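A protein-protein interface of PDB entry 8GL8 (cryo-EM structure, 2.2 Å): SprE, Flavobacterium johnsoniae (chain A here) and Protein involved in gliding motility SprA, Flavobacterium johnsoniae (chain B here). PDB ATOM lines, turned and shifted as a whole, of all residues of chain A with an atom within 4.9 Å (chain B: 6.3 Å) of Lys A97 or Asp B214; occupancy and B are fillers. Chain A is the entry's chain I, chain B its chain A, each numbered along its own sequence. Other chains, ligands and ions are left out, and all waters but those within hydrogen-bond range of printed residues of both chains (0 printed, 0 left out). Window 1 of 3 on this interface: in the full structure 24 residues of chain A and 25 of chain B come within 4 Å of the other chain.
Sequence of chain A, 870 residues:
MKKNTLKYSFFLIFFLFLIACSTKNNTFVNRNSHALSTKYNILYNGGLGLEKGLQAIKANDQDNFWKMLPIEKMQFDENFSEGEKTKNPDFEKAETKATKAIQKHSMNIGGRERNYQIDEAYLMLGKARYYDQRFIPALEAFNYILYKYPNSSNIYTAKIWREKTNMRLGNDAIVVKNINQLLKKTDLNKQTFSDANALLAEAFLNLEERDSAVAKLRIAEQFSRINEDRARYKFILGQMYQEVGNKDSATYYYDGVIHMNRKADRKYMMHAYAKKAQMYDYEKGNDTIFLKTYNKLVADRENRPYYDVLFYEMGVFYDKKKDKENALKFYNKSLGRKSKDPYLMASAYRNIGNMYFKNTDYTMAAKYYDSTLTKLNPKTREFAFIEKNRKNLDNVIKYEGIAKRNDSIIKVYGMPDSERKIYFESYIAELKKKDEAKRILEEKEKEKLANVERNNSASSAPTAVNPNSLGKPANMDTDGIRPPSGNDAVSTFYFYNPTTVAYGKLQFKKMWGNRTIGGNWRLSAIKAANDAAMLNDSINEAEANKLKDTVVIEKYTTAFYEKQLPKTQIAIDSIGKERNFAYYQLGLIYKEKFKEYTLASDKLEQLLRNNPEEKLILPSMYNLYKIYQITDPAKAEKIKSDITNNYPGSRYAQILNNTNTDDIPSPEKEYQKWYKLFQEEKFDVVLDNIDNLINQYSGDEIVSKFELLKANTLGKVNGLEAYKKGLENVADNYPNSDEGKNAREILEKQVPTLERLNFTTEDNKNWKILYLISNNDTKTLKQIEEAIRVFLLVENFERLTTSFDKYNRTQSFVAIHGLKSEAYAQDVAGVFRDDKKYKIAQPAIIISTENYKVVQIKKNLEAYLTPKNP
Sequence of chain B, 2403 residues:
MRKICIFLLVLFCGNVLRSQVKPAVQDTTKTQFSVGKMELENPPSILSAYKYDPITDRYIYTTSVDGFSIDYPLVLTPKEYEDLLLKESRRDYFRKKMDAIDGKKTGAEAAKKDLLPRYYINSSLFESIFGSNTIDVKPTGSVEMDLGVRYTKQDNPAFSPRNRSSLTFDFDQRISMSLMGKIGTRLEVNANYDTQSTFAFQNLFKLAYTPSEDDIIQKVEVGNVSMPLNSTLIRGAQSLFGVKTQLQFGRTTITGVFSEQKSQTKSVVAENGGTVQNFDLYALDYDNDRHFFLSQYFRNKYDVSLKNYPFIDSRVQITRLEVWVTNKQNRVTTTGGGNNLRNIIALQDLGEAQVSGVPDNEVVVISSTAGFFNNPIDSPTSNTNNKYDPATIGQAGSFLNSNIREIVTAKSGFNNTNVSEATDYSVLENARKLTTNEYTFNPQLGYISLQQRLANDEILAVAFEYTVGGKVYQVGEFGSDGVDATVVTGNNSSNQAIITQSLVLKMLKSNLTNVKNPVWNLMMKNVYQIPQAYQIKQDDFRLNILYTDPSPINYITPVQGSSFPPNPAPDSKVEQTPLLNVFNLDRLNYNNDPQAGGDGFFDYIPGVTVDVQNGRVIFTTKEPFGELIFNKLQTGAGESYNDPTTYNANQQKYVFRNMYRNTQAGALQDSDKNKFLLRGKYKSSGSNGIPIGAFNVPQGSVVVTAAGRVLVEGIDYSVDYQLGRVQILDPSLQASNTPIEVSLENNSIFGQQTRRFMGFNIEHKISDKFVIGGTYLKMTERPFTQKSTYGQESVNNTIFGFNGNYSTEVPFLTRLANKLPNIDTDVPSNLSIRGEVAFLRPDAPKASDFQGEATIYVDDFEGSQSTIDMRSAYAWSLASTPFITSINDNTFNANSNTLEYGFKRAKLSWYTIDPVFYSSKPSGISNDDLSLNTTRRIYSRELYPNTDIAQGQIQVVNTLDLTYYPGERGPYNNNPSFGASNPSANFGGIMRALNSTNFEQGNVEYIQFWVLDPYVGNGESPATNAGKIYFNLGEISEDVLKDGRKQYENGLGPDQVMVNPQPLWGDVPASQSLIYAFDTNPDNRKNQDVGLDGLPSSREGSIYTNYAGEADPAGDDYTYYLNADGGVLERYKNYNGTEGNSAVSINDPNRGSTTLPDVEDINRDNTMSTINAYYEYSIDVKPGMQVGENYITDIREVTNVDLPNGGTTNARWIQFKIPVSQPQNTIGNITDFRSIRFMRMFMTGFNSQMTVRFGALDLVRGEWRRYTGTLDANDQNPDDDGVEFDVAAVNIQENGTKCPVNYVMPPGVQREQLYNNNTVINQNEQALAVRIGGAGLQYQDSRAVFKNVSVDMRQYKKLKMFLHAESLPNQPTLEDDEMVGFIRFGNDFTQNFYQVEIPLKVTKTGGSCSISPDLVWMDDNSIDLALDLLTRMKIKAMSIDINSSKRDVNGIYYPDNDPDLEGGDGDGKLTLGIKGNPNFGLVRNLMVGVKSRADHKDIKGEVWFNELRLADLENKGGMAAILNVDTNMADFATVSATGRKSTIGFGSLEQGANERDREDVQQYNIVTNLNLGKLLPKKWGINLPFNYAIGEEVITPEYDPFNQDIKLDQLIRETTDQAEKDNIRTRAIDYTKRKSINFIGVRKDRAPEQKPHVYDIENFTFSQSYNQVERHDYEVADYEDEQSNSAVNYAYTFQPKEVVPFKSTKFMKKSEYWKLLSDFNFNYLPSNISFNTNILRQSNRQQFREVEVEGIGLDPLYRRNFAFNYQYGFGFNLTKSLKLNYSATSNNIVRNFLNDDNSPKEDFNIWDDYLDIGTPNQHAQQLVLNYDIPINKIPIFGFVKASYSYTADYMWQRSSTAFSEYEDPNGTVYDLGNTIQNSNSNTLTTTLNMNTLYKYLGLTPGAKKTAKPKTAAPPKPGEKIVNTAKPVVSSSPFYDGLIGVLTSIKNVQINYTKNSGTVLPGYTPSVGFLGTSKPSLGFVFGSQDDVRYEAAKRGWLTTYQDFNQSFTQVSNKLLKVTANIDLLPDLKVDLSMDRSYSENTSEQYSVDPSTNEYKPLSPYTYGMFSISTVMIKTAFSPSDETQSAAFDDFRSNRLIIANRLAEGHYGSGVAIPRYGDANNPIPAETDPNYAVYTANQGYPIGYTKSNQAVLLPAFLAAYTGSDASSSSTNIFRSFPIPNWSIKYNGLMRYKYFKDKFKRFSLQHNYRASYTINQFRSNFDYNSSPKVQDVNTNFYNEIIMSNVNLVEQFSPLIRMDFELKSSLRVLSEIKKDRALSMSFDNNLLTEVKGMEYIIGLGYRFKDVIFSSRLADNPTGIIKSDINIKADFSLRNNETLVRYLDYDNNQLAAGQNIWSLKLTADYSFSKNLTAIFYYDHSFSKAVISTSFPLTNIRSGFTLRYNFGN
Printed residues of chain B within 4 Å of Ile A42: Asp B214. Printed residues of chain B within 4 Å of Asn A45: Glu B213 and Asp B214. Gly A46 touches none of the printed residues of chain B. Of chain B, only Glu B213 (3.8 Å) and Asp B214 (3.2 Å) come within 4 Å of Lys A97. Asp B214 touches just these residues of chain A: Tyr A40, Asn A41, Ile A42, Asn A45, Lys A97 and Lys A100. Of the printed residues of chain A, Ile B216 touches Tyr A40 and Asn A41. The nearest printed residue of chain B that does not touch Lys A97 is Ser B212 (7.3 Å). The nearest printed residue of chain B that does not touch Tyr A40 is Asp B215 (4.9 Å).
Of the 7 printed residues of chain B, 5 touch a printed residue of chain A. Hydrophobic or aromatic side chains of chain B within 4 Å of the printed part of chain A: Ile B216. Along chain B the printed residues that touch a printed residue of chain A span positions 212 to 216. Of the 16 printed residues of chain A, 6 touch a printed residue of chain B. Among the printed residues, 12 pairs touch across the chains. Among the printed residues, Asp or Glu carboxylates within 4 Å of a Lys or Arg side-chain nitrogen of the other chain: Lys A97 with Glu B213 (3.8 Å), Lys A97 with Asp B214 (3.97 Å) and Lys A100 with Asp B214 (2.4 Å).
The backbone carbonyl oxygen (O) of Asn A41 sits close to the side-chain amide nitrogen (ND2) of Asn A45 (3.3 Å). The side-chain amide nitrogen of Gln B218 sits at hydrogen-bond distance from the backbone carbonyl oxygen of Glu B213, at 3.4 Å. OG of Ser B212 sits at hydrogen-bond distance from OD2 of Asp B215 (2.8 Å). The side-chain hydroxyl of Ser B212 sits close to the backbone NH of Asp B214 (3.4 Å). The backbone carbonyl oxygen of Ser B212 sits at hydrogen-bond distance from the side-chain amide nitrogen of Gln B218 (3.2 Å).
The backbone NH (N) of Asn A41 sits at hydrogen-bond distance from the backbone carbonyl oxygen (O) of Asp B214. The side-chain carboxylate (OD1) of Asp B214 sits at hydrogen-bond distance from the side-chain amide nitrogen (ND2) of Asn A45, 2.6 Å away. The side-chain carboxylate of Glu B213 lies within salt-bridge range of the side-chain amino group of Lys A97, at 3.8 Å. The backbone carbonyl oxygen (O) of Asp B215 is in hydrogen-bond range of the side-chain amide nitrogen (ND2) of Asn A41, at 3.3 Å. The side-chain amino group of Lys A100 lies within salt-bridge range of the side-chain carboxylate of Asp B214 (2.4 Å). OD1 of Asp B214 lies within salt-bridge range of NZ of Lys A97 (3.97 Å). The side-chain amide nitrogen (ND2) of Asn A45 lies within hydrogen-bond range of the backbone carbonyl oxygen (O) of Glu B213.
Among the printed residues, pairs that only touch across the chains: Tyr A40 with Ile B216, Ile A42 with Asp B214, Tyr A40 with Asp B214, Asn A41 with Ile B216 and Lys A100 with Ser B212.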
ATOM      1  N   SER A  37      11.908 -19.059  10.882  1.00  0.00           N
ATOM      2  CA  SER A  37      12.785 -19.304  12.019  1.00  0.00           C
ATOM      3  C   SER A  37      12.742 -20.757  12.471  1.00  0.00           C
ATOM      4  O   SER A  37      13.765 -21.293  12.909  1.00  0.00           O
ATOM      5  CB  SER A  37      12.414 -18.379  13.175  1.00  0.00           C
ATOM      6  OG  SER A  37      12.560 -17.022  12.803  1.00  0.00           O
ATOM      7  N   TYR A  40      14.615 -22.532   9.503  1.00  0.00           N
ATOM      8  CA  TYR A  40      16.023 -22.149   9.549  1.00  0.00           C
ATOM      9  C   TYR A  40      16.307 -21.516  10.905  1.00  0.00           C
ATOM     10  O   TYR A  40      15.790 -20.437  11.210  1.00  0.00           O
ATOM     11  CB  TYR A  40      16.370 -21.180   8.419  1.00  0.00           C
ATOM     12  CG  TYR A  40      15.909 -21.627   7.053  1.00  0.00           C
ATOM     13  CD1 TYR A  40      16.448 -22.753   6.451  1.00  0.00           C
ATOM     14  CD2 TYR A  40      14.940 -20.914   6.361  1.00  0.00           C
ATOM     15  CE1 TYR A  40      16.032 -23.162   5.201  1.00  0.00           C
ATOM     16  CE2 TYR A  40      14.517 -21.315   5.112  1.00  0.00           C
ATOM     17  CZ  TYR A  40      15.066 -22.439   4.536  1.00  0.00           C
ATOM     18  OH  TYR A  40      14.648 -22.842   3.290  1.00  0.00           O
ATOM     19  N   ASN A  41      17.141 -22.170  11.709  1.00  0.00           N
ATOM     20  CA  ASN A  41      17.803 -23.425  11.378  1.00  0.00           C
ATOM     21  C   ASN A  41      17.577 -24.481  12.453  1.00  0.00           C
ATOM     22  O   ASN A  41      18.398 -25.377  12.624  1.00  0.00           O
ATOM     23  CB  ASN A  41      19.306 -23.204  11.184  1.00  0.00           C
ATOM     24  CG  ASN A  41      19.619 -22.344   9.978  1.00  0.00           C
ATOM     25  OD1 ASN A  41      19.486 -22.783   8.837  1.00  0.00           O
ATOM     26  ND2 ASN A  41      20.043 -21.111  10.224  1.00  0.00           N
ATOM     27  N   ILE A  42      16.469 -24.364  13.187  1.00  0.00           N
ATOM     28  CA  ILE A  42      16.167 -25.342  14.227  1.00  0.00           C
ATOM     29  C   ILE A  42      15.884 -26.706  13.609  1.00  0.00           C
ATOM     30  O   ILE A  42      16.485 -27.719  13.988  1.00  0.00           O
ATOM     31  CB  ILE A  42      14.988 -24.864  15.091  1.00  0.00           C
ATOM     32  CG1 ILE A  42      15.161 -23.393  15.468  1.00  0.00           C
ATOM     33  CG2 ILE A  42      14.874 -25.708  16.338  1.00  0.00           C
ATOM     34  CD1 ILE A  42      14.130 -22.896  16.452  1.00  0.00           C
ATOM     35  N   LEU A  43      14.983 -26.747  12.628  1.00  0.00           N
ATOM     36  CA  LEU A  43      14.659 -28.018  11.996  1.00  0.00           C
ATOM     37  C   LEU A  43      15.796 -28.508  11.115  1.00  0.00           C
ATOM     38  O   LEU A  43      15.979 -29.717  10.966  1.00  0.00           O
ATOM     39  CB  LEU A  43      13.368 -27.898  11.190  1.00  0.00           C
ATOM     40  CG  LEU A  43      12.078 -27.838  12.012  1.00  0.00           C
ATOM     41  CD1 LEU A  43      10.866 -28.046  11.125  1.00  0.00           C
ATOM     42  CD2 LEU A  43      12.105 -28.854  13.139  1.00  0.00           C
ATOM     43  N   ASN A  45      19.036 -28.150  11.838  1.00  0.00           N
ATOM     44  CA  ASN A  45      19.968 -28.783  12.766  1.00  0.00           C
ATOM     45  C   ASN A  45      19.409 -30.094  13.302  1.00  0.00           C
ATOM     46  O   ASN A  45      20.154 -31.066  13.487  1.00  0.00           O
ATOM     47  CB  ASN A  45      20.295 -27.829  13.912  1.00  0.00           C
ATOM     48  CG  ASN A  45      21.183 -26.682  13.478  1.00  0.00           C
ATOM     49  OD1 ASN A  45      21.812 -26.735  12.423  1.00  0.00           O
ATOM     50  ND2 ASN A  45      21.239 -25.638  14.291  1.00  0.00           N
ATOM     51  N   GLY A  46      18.100 -30.144  13.558  1.00  0.00           N
ATOM     52  CA  GLY A  46      17.494 -31.397  13.972  1.00  0.00           C
ATOM     53  C   GLY A  46      17.606 -32.477  12.914  1.00  0.00           C
ATOM     54  O   GLY A  46      17.880 -33.637  13.224  1.00  0.00           O
ATOM     55  N   LYS A  93      19.829 -34.842  20.222  1.00  0.00           N
ATOM     56  CA  LYS A  93      19.928 -33.508  19.638  1.00  0.00           C
ATOM     57  C   LYS A  93      18.753 -33.227  18.710  1.00  0.00           C
ATOM     58  O   LYS A  93      18.188 -32.127  18.725  1.00  0.00           O
ATOM     59  CB  LYS A  93      21.250 -33.359  18.887  1.00  0.00           C
ATOM     60  CG  LYS A  93      21.335 -32.098  18.043  1.00  0.00           C
ATOM     61  CD  LYS A  93      22.288 -32.275  16.876  1.00  0.00           C
ATOM     62  CE  LYS A  93      22.496 -30.965  16.134  1.00  0.00           C
ATOM     63  NZ  LYS A  93      23.374 -31.135  14.944  1.00  0.00           N
ATOM     64  N   ALA A  94      18.373 -34.211  17.893  1.00  0.00           N
ATOM     65  CA  ALA A  94      17.225 -34.041  17.008  1.00  0.00           C
ATOM     66  C   ALA A  94      15.943 -33.831  17.800  1.00  0.00           C
ATOM     67  O   ALA A  94      15.114 -32.986  17.442  1.00  0.00           O
ATOM     68  CB  ALA A  94      17.094 -35.249  16.083  1.00  0.00           C
ATOM     69  N   GLU A  95      15.758 -34.595  18.878  1.00  0.00           N
ATOM     70  CA  GLU A  95      14.571 -34.430  19.712  1.00  0.00           C
ATOM     71  C   GLU A  95      14.552 -33.066  20.389  1.00  0.00           C
ATOM     72  O   GLU A  95      13.498 -32.426  20.477  1.00  0.00           O
ATOM     73  CB  GLU A  95      14.503 -35.546  20.751  1.00  0.00           C
ATOM     74  CG  GLU A  95      13.264 -35.494  21.621  1.00  0.00           C
ATOM     75  CD  GLU A  95      13.036 -36.774  22.390  1.00  0.00           C
ATOM     76  OE1 GLU A  95      13.739 -37.767  22.111  1.00  0.00           O
ATOM     77  OE2 GLU A  95      12.154 -36.789  23.272  1.00  0.00           O
ATOM     78  N   THR A  96      15.706 -32.608  20.877  1.00  0.00           N
ATOM     79  CA  THR A  96      15.785 -31.288  21.490  1.00  0.00           C
ATOM     80  C   THR A  96      15.460 -30.194  20.481  1.00  0.00           C
ATOM     81  O   THR A  96      14.747 -29.238  20.800  1.00  0.00           O
ATOM     82  CB  THR A  96      17.175 -31.071  22.085  1.00  0.00           C
ATOM     83  OG1 THR A  96      17.405 -32.033  23.120  1.00  0.00           O
ATOM     84  CG2 THR A  96      17.300 -29.675  22.665  1.00  0.00           C
ATOM     85  N   LYS A  97      15.975 -30.318  19.257  1.00  0.00           N
ATOM     86  CA  LYS A  97      15.676 -29.330  18.227  1.00  0.00           C
ATOM     87  C   LYS A  97      14.198 -29.339  17.859  1.00  0.00           C
ATOM     88  O   LYS A  97      13.594 -28.279  17.677  1.00  0.00           O
ATOM     89  CB  LYS A  97      16.540 -29.576  16.994  1.00  0.00           C
ATOM     90  CG  LYS A  97      17.994 -29.191  17.178  1.00  0.00           C
ATOM     91  CD  LYS A  97      18.121 -27.788  17.734  1.00  0.00           C
ATOM     92  CE  LYS A  97      19.449 -27.594  18.440  1.00  0.00           C
ATOM     93  NZ  LYS A  97      20.426 -28.654  18.079  1.00  0.00           N
ATOM     94  N   ALA A  98      13.598 -30.524  17.743  1.00  0.00           N
ATOM     95  CA  ALA A  98      12.172 -30.597  17.442  1.00  0.00           C
ATOM     96  C   ALA A  98      11.340 -29.978  18.560  1.00  0.00           C
ATOM     97  O   ALA A  98      10.360 -29.270  18.297  1.00  0.00           O
ATOM     98  CB  ALA A  98      11.763 -32.047  17.202  1.00  0.00           C
ATOM     99  N   THR A  99      11.715 -30.236  19.814  1.00  0.00           N
ATOM    100  CA  THR A  99      11.021 -29.627  20.943  1.00  0.00           C
ATOM    101  C   THR A  99      11.160 -28.110  20.920  1.00  0.00           C
ATOM    102  O   THR A  99      10.183 -27.382  21.119  1.00  0.00           O
ATOM    103  CB  THR A  99      11.558 -30.197  22.255  1.00  0.00           C
ATOM    104  OG1 THR A  99      11.441 -31.625  22.241  1.00  0.00           O
ATOM    105  CG2 THR A  99      10.784 -29.647  23.435  1.00  0.00           C
ATOM    106  N   LYS A 100      12.373 -27.615  20.662  1.00  0.00           N
ATOM    107  CA  LYS A 100      12.599 -26.175  20.591  1.00  0.00           C
ATOM    108  C   LYS A 100      11.859 -25.545  19.421  1.00  0.00           C
ATOM    109  O   LYS A 100      11.543 -24.353  19.458  1.00  0.00           O
ATOM    110  CB  LYS A 100      14.098 -25.886  20.494  1.00  0.00           C
ATOM    111  CG  LYS A 100      14.463 -24.411  20.539  1.00  0.00           C
ATOM    112  CD  LYS A 100      15.641 -24.092  19.647  1.00  0.00           C
ATOM    113  CE  LYS A 100      16.426 -22.910  20.189  1.00  0.00           C
ATOM    114  NZ  LYS A 100      17.851 -22.961  19.768  1.00  0.00           N
ATOM    115  N   ALA A 101      11.602 -26.311  18.366  1.00  0.00           N
ATOM    116  CA  ALA A 101      10.806 -25.787  17.264  1.00  0.00           C
ATOM    117  C   ALA A 101       9.324 -25.757  17.610  1.00  0.00           C
ATOM    118  O   ALA A 101       8.622 -24.809  17.246  1.00  0.00           O
ATOM    119  CB  ALA A 101      11.045 -26.612  16.002  1.00  0.00           C
ATOM    120  N   PRO B 211      25.289 -15.703  17.909  1.00  0.00           N
ATOM    121  CA  PRO B 211      24.098 -16.340  18.484  1.00  0.00           C
ATOM    122  C   PRO B 211      24.181 -17.857  18.479  1.00  0.00           C
ATOM    123  O   PRO B 211      25.220 -18.432  18.139  1.00  0.00           O
ATOM    124  CB  PRO B 211      22.957 -15.842  17.582  1.00  0.00           C
ATOM    125  CG  PRO B 211      23.550 -14.749  16.741  1.00  0.00           C
ATOM    126  CD  PRO B 211      25.000 -15.057  16.621  1.00  0.00           C
ATOM    127  N   SER B 212      23.087 -18.513  18.858  1.00  0.00           N
ATOM    128  CA  SER B 212      23.045 -19.965  18.863  1.00  0.00           C
ATOM    129  C   SER B 212      23.072 -20.508  17.436  1.00  0.00           C
ATOM    130  O   SER B 212      22.843 -19.788  16.460  1.00  0.00           O
ATOM    131  CB  SER B 212      21.797 -20.465  19.592  1.00  0.00           C
ATOM    132  OG  SER B 212      20.655 -20.389  18.757  1.00  0.00           O
ATOM    133  N   GLU B 213      23.360 -21.806  17.326  1.00  0.00           N
ATOM    134  CA  GLU B 213      23.486 -22.442  16.020  1.00  0.00           C
ATOM    135  C   GLU B 213      22.166 -22.505  15.264  1.00  0.00           C
ATOM    136  O   GLU B 213      22.177 -22.722  14.048  1.00  0.00           O
ATOM    137  CB  GLU B 213      24.056 -23.852  16.180  1.00  0.00           C
ATOM    138  CG  GLU B 213      23.337 -24.691  17.222  1.00  0.00           C
ATOM    139  CD  GLU B 213      23.700 -26.160  17.141  1.00  0.00           C
ATOM    140  OE1 GLU B 213      23.913 -26.661  16.017  1.00  0.00           O
ATOM    141  OE2 GLU B 213      23.772 -26.815  18.201  1.00  0.00           O
ATOM    142  N   ASP B 214      21.038 -22.324  15.945  1.00  0.00           N
ATOM    143  CA  ASP B 214      19.727 -22.442  15.322  1.00  0.00           C
ATOM    144  C   ASP B 214      19.202 -21.126  14.765  1.00  0.00           C
ATOM    145  O   ASP B 214      18.123 -21.114  14.163  1.00  0.00           O
ATOM    146  CB  ASP B 214      18.720 -23.008  16.326  1.00  0.00           C
ATOM    147  CG  ASP B 214      19.228 -24.254  17.016  1.00  0.00           C
ATOM    148  OD1 ASP B 214      19.688 -25.175  16.311  1.00  0.00           O
ATOM    149  OD2 ASP B 214      19.167 -24.314  18.261  1.00  0.00           O
ATOM    150  N   ASP B 215      19.926 -20.027  14.943  1.00  0.00           N
ATOM    151  CA  ASP B 215      19.471 -18.725  14.483  1.00  0.00           C
ATOM    152  C   ASP B 215      19.868 -18.498  13.030  1.00  0.00           C
ATOM    153  O   ASP B 215      20.894 -18.997  12.560  1.00  0.00           O
ATOM    154  CB  ASP B 215      20.045 -17.613  15.360  1.00  0.00           C
ATOM    155  CG  ASP B 215      19.353 -17.515  16.706  1.00  0.00           C
ATOM    156  OD1 ASP B 215      18.182 -17.084  16.742  1.00  0.00           O
ATOM    157  OD2 ASP B 215      19.978 -17.868  17.726  1.00  0.00           O
ATOM    158  N   ILE B 216      19.030 -17.744  12.315  1.00  0.00           N
ATOM    159  CA  ILE B 216      19.359 -17.368  10.942  1.00  0.00           C
ATOM    160  C   ILE B 216      20.610 -16.501  10.920  1.00  0.00           C
ATOM    161  O   ILE B 216      21.529 -16.719  10.122  1.00  0.00           O
ATOM    162  CB  ILE B 216      18.166 -16.658  10.278  1.00  0.00           C
ATOM    163  CG1 ILE B 216      17.060 -17.662   9.956  1.00  0.00           C
ATOM    164  CG2 ILE B 216      18.609 -15.937   9.016  1.00  0.00           C
ATOM    165  CD1 ILE B 216      15.742 -17.020   9.598  1.00  0.00           C
ATOM    166  N   GLN B 218      23.990 -15.836  12.125  1.00  0.00           N
ATOM    167  CA  GLN B 218      25.014 -16.649  12.764  1.00  0.00           C
ATOM    168  C   GLN B 218      26.169 -15.835  13.328  1.00  0.00           C
ATOM    169  O   GLN B 218      26.852 -16.313  14.239  1.00  0.00           O
ATOM    170  CB  GLN B 218      25.569 -17.677  11.772  1.00  0.00           C
ATOM    171  CG  GLN B 218      24.700 -18.911  11.606  1.00  0.00           C
ATOM    172  CD  GLN B 218      24.335 -19.546  12.932  1.00  0.00           C
ATOM    173  OE1 GLN B 218      25.192 -20.080  13.633  1.00  0.00           O
ATOM    174  NE2 GLN B 218      23.058 -19.487  13.283  1.00  0.00           N
